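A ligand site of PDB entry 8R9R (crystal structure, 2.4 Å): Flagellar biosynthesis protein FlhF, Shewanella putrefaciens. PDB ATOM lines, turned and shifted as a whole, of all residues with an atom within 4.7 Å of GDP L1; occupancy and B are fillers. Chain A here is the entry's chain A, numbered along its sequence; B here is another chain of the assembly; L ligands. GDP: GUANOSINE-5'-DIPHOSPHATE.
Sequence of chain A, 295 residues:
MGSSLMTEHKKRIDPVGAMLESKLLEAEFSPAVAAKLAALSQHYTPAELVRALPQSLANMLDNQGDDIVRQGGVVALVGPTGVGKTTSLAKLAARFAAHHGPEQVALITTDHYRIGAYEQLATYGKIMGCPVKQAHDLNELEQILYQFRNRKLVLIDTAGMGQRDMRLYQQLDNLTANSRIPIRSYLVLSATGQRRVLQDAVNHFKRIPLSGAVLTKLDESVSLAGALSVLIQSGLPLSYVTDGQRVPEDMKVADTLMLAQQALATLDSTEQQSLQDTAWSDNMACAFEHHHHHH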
ATOM      1  N   PRO A  80       9.495 -13.999 -22.969  1.00  0.00           N
ATOM      2  CA  PRO A  80      10.535 -14.513 -22.082  1.00  0.00           C
ATOM      3  C   PRO A  80      10.469 -16.038 -21.991  1.00  0.00           C
ATOM      4  O   PRO A  80       9.646 -16.662 -22.657  1.00  0.00           O
ATOM      5  CB  PRO A  80      10.267 -13.787 -20.760  1.00  0.00           C
ATOM      6  CG  PRO A  80       8.801 -13.422 -20.796  1.00  0.00           C
ATOM      7  CD  PRO A  80       8.390 -13.331 -22.253  1.00  0.00           C
ATOM      8  N   THR A  81      11.344 -16.615 -21.172  1.00  0.00           N
ATOM      9  CA  THR A  81      11.600 -18.050 -21.166  1.00  0.00           C
ATOM     10  C   THR A  81      10.467 -18.911 -20.615  1.00  0.00           C
ATOM     11  O   THR A  81       9.828 -18.544 -19.632  1.00  0.00           O
ATOM     12  CB  THR A  81      12.859 -18.293 -20.367  1.00  0.00           C
ATOM     13  OG1 THR A  81      12.707 -17.757 -19.043  1.00  0.00           O
ATOM     14  CG2 THR A  81      14.087 -17.663 -21.011  1.00  0.00           C
ATOM     15  N   GLY A  82      10.221 -20.055 -21.266  1.00  0.00           N
ATOM     16  CA  GLY A  82       9.324 -21.082 -20.758  1.00  0.00           C
ATOM     17  C   GLY A  82       7.847 -20.709 -20.682  1.00  0.00           C
ATOM     18  O   GLY A  82       7.046 -21.409 -20.066  1.00  0.00           O
ATOM     19  N   VAL A  83       7.478 -19.606 -21.335  1.00  0.00           N
ATOM     20  CA  VAL A  83       6.106 -19.133 -21.331  1.00  0.00           C
ATOM     21  C   VAL A  83       5.198 -19.959 -22.246  1.00  0.00           C
ATOM     22  O   VAL A  83       3.976 -19.937 -22.073  1.00  0.00           O
ATOM     23  CB  VAL A  83       6.057 -17.631 -21.703  1.00  0.00           C
ATOM     24  CG1 VAL A  83       6.778 -16.778 -20.648  1.00  0.00           C
ATOM     25  CG2 VAL A  83       6.618 -17.369 -23.107  1.00  0.00           C
ATOM     26  N   GLY A  84       5.788 -20.676 -23.208  1.00  0.00           N
ATOM     27  CA  GLY A  84       5.042 -21.557 -24.093  1.00  0.00           C
ATOM     28  C   GLY A  84       4.934 -21.099 -25.544  1.00  0.00           C
ATOM     29  O   GLY A  84       3.919 -21.335 -26.199  1.00  0.00           O
ATOM     30  N   LYS A  85       5.973 -20.409 -26.038  1.00  0.00           N
ATOM     31  CA  LYS A  85       6.017 -19.946 -27.417  1.00  0.00           C
ATOM     32  C   LYS A  85       5.941 -21.102 -28.407  1.00  0.00           C
ATOM     33  O   LYS A  85       5.134 -21.076 -29.332  1.00  0.00           O
ATOM     34  CB  LYS A  85       7.296 -19.128 -27.694  1.00  0.00           C
ATOM     35  CG  LYS A  85       7.370 -17.801 -26.963  1.00  0.00           C
ATOM     36  CD  LYS A  85       8.632 -16.957 -27.308  1.00  0.00           C
ATOM     37  CE  LYS A  85       9.954 -17.664 -27.036  1.00  0.00           C
ATOM     38  NZ  LYS A  85      10.077 -18.100 -25.598  1.00  0.00           N
ATOM     39  N   THR A  86       6.778 -22.136 -28.198  1.00  0.00           N
ATOM     40  CA  THR A  86       6.817 -23.278 -29.101  1.00  0.00           C
ATOM     41  C   THR A  86       5.486 -24.042 -29.084  1.00  0.00           C
ATOM     42  O   THR A  86       4.987 -24.449 -30.140  1.00  0.00           O
ATOM     43  CB  THR A  86       7.985 -24.203 -28.758  1.00  0.00           C
ATOM     44  OG1 THR A  86       9.185 -23.441 -28.728  1.00  0.00           O
ATOM     45  CG2 THR A  86       8.144 -25.321 -29.754  1.00  0.00           C
ATOM     46  N   THR A  87       4.938 -24.235 -27.885  1.00  0.00           N
ATOM     47  CA  THR A  87       3.684 -24.944 -27.692  1.00  0.00           C
ATOM     48  C   THR A  87       2.498 -24.211 -28.300  1.00  0.00           C
ATOM     49  O   THR A  87       1.604 -24.826 -28.877  1.00  0.00           O
ATOM     50  CB  THR A  87       3.490 -25.179 -26.202  1.00  0.00           C
ATOM     51  OG1 THR A  87       4.668 -25.799 -25.685  1.00  0.00           O
ATOM     52  CG2 THR A  87       2.300 -26.031 -25.899  1.00  0.00           C
ATOM     53  N   LYS A  91       0.029 -25.073 -31.663  1.00  0.00           N
ATOM     54  CA  LYS A  91      -1.424 -24.984 -31.575  1.00  0.00           C
ATOM     55  C   LYS A  91      -1.975 -24.129 -32.706  1.00  0.00           C
ATOM     56  O   LYS A  91      -2.955 -24.499 -33.341  1.00  0.00           O
ATOM     57  CB  LYS A  91      -1.843 -24.423 -30.205  1.00  0.00           C
ATOM     58  CG  LYS A  91      -1.573 -25.392 -29.047  1.00  0.00           C
ATOM     59  CD  LYS A  91      -1.689 -24.758 -27.678  1.00  0.00           C
ATOM     60  CE  LYS A  91      -1.375 -25.738 -26.576  1.00  0.00           C
ATOM     61  NZ  LYS A  91      -1.682 -25.165 -25.213  1.00  0.00           N
ATOM     62  N   ARG A 114      18.797 -23.262 -27.841  1.00  0.00           N
ATOM     63  CA  ARG A 114      18.341 -24.478 -27.181  1.00  0.00           C
ATOM     64  C   ARG A 114      18.919 -25.743 -27.799  1.00  0.00           C
ATOM     65  O   ARG A 114      19.056 -25.825 -29.025  1.00  0.00           O
ATOM     66  CB  ARG A 114      16.808 -24.621 -27.229  1.00  0.00           C
ATOM     67  CG  ARG A 114      16.042 -23.475 -26.617  1.00  0.00           C
ATOM     68  CD  ARG A 114      16.335 -23.279 -25.138  1.00  0.00           C
ATOM     69  NE  ARG A 114      15.485 -22.249 -24.566  1.00  0.00           N
ATOM     70  CZ  ARG A 114      15.460 -20.983 -24.960  1.00  0.00           C
ATOM     71  NH1 ARG A 114      16.444 -20.464 -25.684  1.00  0.00           N
ATOM     72  NH2 ARG A 114      14.443 -20.210 -24.597  1.00  0.00           N
ATOM     73  N   THR A 216      -0.748 -17.339 -21.685  1.00  0.00           N
ATOM     74  CA  THR A 216      -0.631 -18.767 -21.427  1.00  0.00           C
ATOM     75  C   THR A 216      -0.827 -19.127 -19.965  1.00  0.00           C
ATOM     76  O   THR A 216      -0.730 -18.282 -19.078  1.00  0.00           O
ATOM     77  CB  THR A 216       0.718 -19.265 -21.921  1.00  0.00           C
ATOM     78  OG1 THR A 216       1.756 -18.607 -21.175  1.00  0.00           O
ATOM     79  CG2 THR A 216       0.919 -19.043 -23.423  1.00  0.00           C
ATOM     80  N   LYS A 217      -1.110 -20.421 -19.746  1.00  0.00           N
ATOM     81  CA  LYS A 217      -1.099 -21.039 -18.423  1.00  0.00           C
ATOM     82  C   LYS A 217      -2.192 -20.491 -17.512  1.00  0.00           C
ATOM     83  O   LYS A 217      -1.969 -20.292 -16.329  1.00  0.00           O
ATOM     84  CB  LYS A 217       0.281 -20.899 -17.774  1.00  0.00           C
ATOM     85  CG  LYS A 217       1.408 -21.275 -18.702  1.00  0.00           C
ATOM     86  CD  LYS A 217       2.711 -21.516 -18.003  1.00  0.00           C
ATOM     87  CE  LYS A 217       3.797 -21.850 -18.999  1.00  0.00           C
ATOM     88  NZ  LYS A 217       5.060 -22.219 -18.332  1.00  0.00           N
ATOM     89  N   ASP A 219      -4.595 -22.304 -16.664  1.00  0.00           N
ATOM     90  CA  ASP A 219      -4.784 -23.452 -15.788  1.00  0.00           C
ATOM     91  C   ASP A 219      -3.833 -23.498 -14.596  1.00  0.00           C
ATOM     92  O   ASP A 219      -4.070 -24.263 -13.662  1.00  0.00           O
ATOM     93  CB  ASP A 219      -4.659 -24.741 -16.609  1.00  0.00           C
ATOM     94  CG  ASP A 219      -3.285 -24.946 -17.220  1.00  0.00           C
ATOM     95  OD1 ASP A 219      -2.810 -24.045 -17.948  1.00  0.00           O
ATOM     96  OD2 ASP A 219      -2.676 -26.010 -16.964  1.00  0.00           O
ATOM     97  N   GLU A 220      -2.750 -22.703 -14.623  1.00  0.00           N
ATOM     98  CA  GLU A 220      -1.841 -22.552 -13.491  1.00  0.00           C
ATOM     99  C   GLU A 220      -2.061 -21.273 -12.685  1.00  0.00           C
ATOM    100  O   GLU A 220      -1.452 -21.092 -11.626  1.00  0.00           O
ATOM    101  CB  GLU A 220      -0.387 -22.536 -13.986  1.00  0.00           C
ATOM    102  CG  GLU A 220       0.196 -23.909 -14.285  1.00  0.00           C
ATOM    103  CD  GLU A 220       1.644 -23.913 -14.730  1.00  0.00           C
ATOM    104  OE1 GLU A 220       2.411 -23.035 -14.270  1.00  0.00           O
ATOM    105  OE2 GLU A 220       2.028 -24.815 -15.516  1.00  0.00           O
ATOM    106  N   THR A 242      -4.238 -19.760 -23.655  1.00  0.00           N
ATOM    107  CA  THR A 242      -4.008 -21.197 -23.570  1.00  0.00           C
ATOM    108  C   THR A 242      -4.229 -21.617 -22.123  1.00  0.00           C
ATOM    109  O   THR A 242      -3.948 -20.856 -21.209  1.00  0.00           O
ATOM    110  CB  THR A 242      -2.602 -21.566 -24.100  1.00  0.00           C
ATOM    111  OG1 THR A 242      -1.602 -21.295 -23.115  1.00  0.00           O
ATOM    112  CG2 THR A 242      -2.266 -20.839 -25.404  1.00  0.00           C
ATOM    113  N   ASP A 243      -4.735 -22.835 -21.947  1.00  0.00           N
ATOM    114  CA  ASP A 243      -5.188 -23.322 -20.650  1.00  0.00           C
ATOM    115  C   ASP A 243      -4.796 -24.778 -20.415  1.00  0.00           C
ATOM    116  O   ASP A 243      -5.472 -25.486 -19.666  1.00  0.00           O
ATOM    117  CB  ASP A 243      -6.720 -23.161 -20.559  1.00  0.00           C
ATOM    118  CG  ASP A 243      -7.486 -23.845 -21.661  1.00  0.00           C
ATOM    119  OD1 ASP A 243      -6.841 -24.499 -22.546  1.00  0.00           O
ATOM    120  OD2 ASP A 243      -8.731 -23.754 -21.667  1.00  0.00           O
ATOM    121  N   GLY A 244      -3.695 -25.208 -21.036  1.00  0.00           N
ATOM    122  CA  GLY A 244      -3.152 -26.524 -20.776  1.00  0.00           C
ATOM    123  C   GLY A 244      -2.037 -26.893 -21.750  1.00  0.00           C
ATOM    124  O   GLY A 244      -1.638 -26.085 -22.583  1.00  0.00           O
ATOM    125  N   GLN A 245      -1.556 -28.136 -21.620  1.00  0.00           N
ATOM    126  CA  GLN A 245      -0.400 -28.597 -22.363  1.00  0.00           C
ATOM    127  C   GLN A 245      -0.773 -29.398 -23.606  1.00  0.00           C
ATOM    128  O   GLN A 245       0.112 -29.812 -24.359  1.00  0.00           O
ATOM    129  CB  GLN A 245       0.482 -29.446 -21.444  1.00  0.00           C
ATOM    130  CG  GLN A 245       1.139 -28.646 -20.325  1.00  0.00           C
ATOM    131  CD  GLN A 245       2.025 -29.526 -19.497  1.00  0.00           C
ATOM    132  OE1 GLN A 245       1.556 -30.261 -18.625  1.00  0.00           O
ATOM    133  NE2 GLN A 245       3.325 -29.472 -19.748  1.00  0.00           N
ATOM    134  N   THR B  81       5.540 -25.947 -14.989  1.00  0.00           N
ATOM    135  CA  THR B  81       6.099 -25.907 -16.334  1.00  0.00           C
ATOM    136  C   THR B  81       7.062 -24.753 -16.605  1.00  0.00           C
ATOM    137  O   THR B  81       6.830 -23.632 -16.159  1.00  0.00           O
ATOM    138  CB  THR B  81       4.950 -25.850 -17.313  1.00  0.00           C
ATOM    139  OG1 THR B  81       4.122 -24.712 -17.028  1.00  0.00           O
ATOM    140  CG2 THR B  81       4.087 -27.104 -17.269  1.00  0.00           C
ATOM    141  N   GLY B  82       8.147 -25.045 -17.332  1.00  0.00           N
ATOM    142  CA  GLY B  82       9.051 -24.031 -17.854  1.00  0.00           C
ATOM    143  C   GLY B  82       9.852 -23.248 -16.819  1.00  0.00           C
ATOM    144  O   GLY B  82      10.467 -22.229 -17.129  1.00  0.00           O
ATOM    145  N   ARG B 114       7.079 -34.678 -23.089  1.00  0.00           N
ATOM    146  CA  ARG B 114       7.698 -33.740 -24.016  1.00  0.00           C
ATOM    147  C   ARG B 114       8.254 -34.416 -25.262  1.00  0.00           C
ATOM    148  O   ARG B 114       8.810 -35.517 -25.172  1.00  0.00           O
ATOM    149  CB  ARG B 114       8.865 -32.973 -23.369  1.00  0.00           C
ATOM    150  CG  ARG B 114       8.505 -32.192 -22.129  1.00  0.00           C
ATOM    151  CD  ARG B 114       7.465 -31.111 -22.383  1.00  0.00           C
ATOM    152  NE  ARG B 114       7.242 -30.307 -21.194  1.00  0.00           N
ATOM    153  CZ  ARG B 114       6.801 -30.776 -20.034  1.00  0.00           C
ATOM    154  NH1 ARG B 114       6.206 -31.960 -19.948  1.00  0.00           N
ATOM    155  NH2 ARG B 114       6.932 -30.034 -18.941  1.00  0.00           N
ATOM    156  N   GLY B 160       7.448 -31.379 -16.177  1.00  0.00           N
ATOM    157  CA  GLY B 160       6.738 -30.173 -15.781  1.00  0.00           C
ATOM    158  C   GLY B 160       5.242 -30.274 -16.054  1.00  0.00           C
ATOM    159  O   GLY B 160       4.826 -30.587 -17.173  1.00  0.00           O
ATOM    160  N   GLY B 162       1.246 -28.364 -14.663  1.00  0.00           N
ATOM    161  CA  GLY B 162       0.528 -27.409 -13.838  1.00  0.00           C
ATOM    162  C   GLY B 162       0.238 -27.986 -12.459  1.00  0.00           C
ATOM    163  O   GLY B 162      -0.117 -29.161 -12.329  1.00  0.00           O
HETATM  164  PB  GDP L   1       8.997 -21.788 -24.735  1.00  0.00           P
HETATM  165  O1B GDP L   1      10.310 -22.111 -24.069  1.00  0.00           O
HETATM  166  O2B GDP L   1       8.679 -20.330 -24.660  1.00  0.00           O
HETATM  167  O3B GDP L   1       8.952 -22.184 -26.167  1.00  0.00           O
HETATM  168  O3A GDP L   1       7.901 -22.673 -23.932  1.00  0.00           O
HETATM  169  PA  GDP L   1       7.506 -24.163 -24.517  1.00  0.00           P
HETATM  170  O1A GDP L   1       6.535 -24.021 -25.710  1.00  0.00           O
HETATM  171  O2A GDP L   1       8.777 -24.920 -24.898  1.00  0.00           O
HETATM  172  O5' GDP L   1       6.733 -24.893 -23.272  1.00  0.00           O
HETATM  173  C5' GDP L   1       7.231 -24.576 -22.029  1.00  0.00           C
HETATM  174  C4' GDP L   1       6.600 -25.495 -21.018  1.00  0.00           C
HETATM  175  O4' GDP L   1       5.216 -24.751 -20.630  1.00  0.00           O
HETATM  176  C3' GDP L   1       6.295 -26.687 -21.482  1.00  0.00           C
HETATM  177  O3' GDP L   1       6.318 -27.675 -20.393  1.00  0.00           O
HETATM  178  C2' GDP L   1       4.802 -26.572 -21.978  1.00  0.00           C
HETATM  179  O2' GDP L   1       4.174 -27.766 -21.902  1.00  0.00           O
HETATM  180  C1' GDP L   1       4.265 -25.648 -20.886  1.00  0.00           C
HETATM  181  N9  GDP L   1       2.993 -24.942 -21.236  1.00  0.00           N
HETATM  182  C8  GDP L   1       2.973 -24.219 -22.377  1.00  0.00           C
HETATM  183  N7  GDP L   1       1.732 -23.670 -22.435  1.00  0.00           N
HETATM  184  C5  GDP L   1       1.053 -24.058 -21.348  1.00  0.00           C
HETATM  185  C6  GDP L   1      -0.352 -23.811 -20.816  1.00  0.00           C
HETATM  186  O6  GDP L   1      -1.127 -23.146 -21.400  1.00  0.00           O
HETATM  187  N1  GDP L   1      -0.731 -24.414 -19.557  1.00  0.00           N
HETATM  188  C2  GDP L   1       0.195 -25.233 -18.829  1.00  0.00           C
HETATM  189  N2  GDP L   1      -0.105 -25.897 -17.537  1.00  0.00           N
HETATM  190  N3  GDP L   1       1.498 -25.454 -19.325  1.00  0.00           N
HETATM  191  C4  GDP L   1       1.860 -24.838 -20.624  1.00  0.00           C
HETATM  192  PB  GDP L   2      11.617 -27.153 -17.553  1.00  0.00           P
HETATM  193  O1B GDP L   2      10.537 -27.229 -18.601  1.00  0.00           O
HETATM  194  O2B GDP L   2      11.049 -27.096 -16.172  1.00  0.00           O
HETATM  195  O3B GDP L   2      12.564 -28.299 -17.601  1.00  0.00           O
HETATM  196  O3A GDP L   2      12.441 -25.803 -17.909  1.00  0.00           O
HETATM  197  PA  GDP L   2      13.776 -25.921 -18.868  1.00  0.00           P
HETATM  198  O1A GDP L   2      14.972 -26.448 -18.046  1.00  0.00           O
HETATM  199  O2A GDP L   2      13.469 -26.812 -20.070  1.00  0.00           O
HETATM  200  O5' GDP L   2      14.075 -24.380 -19.335  1.00  0.00           O
HETATM  201  C5' GDP L   2      12.947 -23.620 -19.544  1.00  0.00           C
HETATM  202  C4' GDP L   2      13.361 -22.329 -20.197  1.00  0.00           C
HETATM  203  O4' GDP L   2      13.750 -21.373 -18.951  1.00  0.00           O
HETATM  204  C3' GDP L   2      14.420 -22.427 -20.972  1.00  0.00           C
HETATM  205  O3' GDP L   2      14.374 -21.399 -22.023  1.00  0.00           O
HETATM  206  C2' GDP L   2      15.648 -22.090 -20.042  1.00  0.00           C
HETATM  207  O2' GDP L   2      16.666 -21.561 -20.756  1.00  0.00           O
HETATM  208  C1' GDP L   2      15.004 -20.994 -19.193  1.00  0.00           C
HETATM  209  N9  GDP L   2      15.701 -20.716 -17.899  1.00  0.00           N
HETATM  210  C8  GDP L   2      15.908 -21.758 -17.064  1.00  0.00           C
HETATM  211  N7  GDP L   2      16.519 -21.230 -15.972  1.00  0.00           N
HETATM  212  C5  GDP L   2      16.654 -19.912 -16.166  1.00  0.00           C
HETATM  213  C6  GDP L   2      17.244 -18.764 -15.358  1.00  0.00           C
HETATM  214  O6  GDP L   2      17.731 -18.936 -14.301  1.00  0.00           O
HETATM  215  N1  GDP L   2      17.195 -17.430 -15.914  1.00  0.00           N
HETATM  216  C2  GDP L   2      16.610 -17.195 -17.204  1.00  0.00           C
HETATM  217  N2  GDP L   2      16.522 -15.867 -17.857  1.00  0.00           N
HETATM  218  N3  GDP L   2      16.061 -18.263 -17.946  1.00  0.00           N
HETATM  219  C4  GDP L   2      16.134 -19.624 -17.362  1.00  0.00           C
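The backbone NH of Thr 87 is in hydrogen-bond range of an oxygen (O1A) of GDP L1.
NH2 of Arg 114 of chain A lies within hydrogen-bond range of O3' of GDP L2, at 2.8 Å.
N2 of GDP L1 sits at hydrogen-bond distance from OD2 of Asp 219 (2.6 Å).
The side-chain hydroxyl of Thr 86 sits at hydrogen-bond distance from an oxygen (O3B) of GDP L1 (2.9 Å).
An oxygen (O4') of GDP L1 lies within hydrogen-bond range of the side-chain amino group (NZ) of Lys 217, 3.4 Å away.
N of Lys 85 sits at hydrogen-bond distance from O2B of GDP L1 (3.0 Å).
An oxygen (O6) of GDP L1 sits at hydrogen-bond distance from the backbone NH (N) of Gly 244, at 3.3 Å.
N of Gly 84 is in hydrogen-bond range of O3A of GDP L1 (3.0 Å).
OE2 of Glu 220 is in hydrogen-bond range of N2 of GDP L1 (3.1 Å).
N of Gly 82 of chain A lies within hydrogen-bond range of O1B of GDP L1 (3.5 Å).
NH2 of Arg 114 of chain B is in hydrogen-bond range of O3' of GDP L1 (2.8 Å).
The backbone NH of Lys 217 is in hydrogen-bond range of an oxygen (O6) of GDP L1, at 3.2 Å.
An oxygen (O3B) of GDP L1 sits at hydrogen-bond distance from the backbone NH (N) of Thr 86, 3.0 Å away.
O1A of GDP L1 is in hydrogen-bond range of OG1 of Thr 87 (2.6 Å).
The side-chain amide nitrogen (NE2) of Gln 245 lies within hydrogen-bond range of an oxygen (O2') of GDP L1.
An oxygen (O1B) of GDP L2 lies within hydrogen-bond range of the backbone NH (N) of Gly 82 of chain B (3.5 Å).
O6 of GDP L1 lies within hydrogen-bond range of OG1 of Thr 242, at 2.6 Å.
NZ of Lys 85 lies within salt-bridge range of O2B of GDP L1 (2.8 Å).
NE2 of Gln 245 sits at hydrogen-bond distance from O of Gly 160 of chain B.
NZ of Lys 217 lies within hydrogen-bond range of O of Gly 82 of chain A (2.8 Å).
O of Gly 244 lies within hydrogen-bond range of NZ of Lys 91 (2.8 Å).
The side-chain carboxylate (OE2) of Glu 220 is in hydrogen-bond range of the side-chain hydroxyl (OG1) of Thr 81 of chain B (2.6 Å).
The backbone carbonyl oxygen (O) of Thr 242 lies within hydrogen-bond range of the backbone NH (N) of Lys 217 (3.2 Å).
O of Pro 80 lies within hydrogen-bond range of NZ of Lys 85 (3.3 Å).
NZ of Lys 217 lies within hydrogen-bond range of OG1 of Thr 81 of chain B, at 3.0 Å.
The side-chain carboxylate of Asp 219 lies within hydrogen-bond range of the backbone NH of Gly 244, at 3.4 Å.
Val 83 touches GDP L1 (N to O2B, 3.6 Å).
Asp 243 touches GDP L1.
Thr 81 of chain B touches GDP L1 (CB to O4', 3.5 Å).
Within 4 Å of GDP L1: Gly 82 of chain A, Val 83, Gly 84, Lys 85, Thr 86, Thr 87, Lys 217, Asp 219, Glu 220, Thr 242, Asp 243, Gly 244, Gln 245, Thr 81 of chain B and Arg 114 of chain B.
The nearest printed residue that does not touch GDP L1 is Gly 162 of chain B (4.02 Å).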
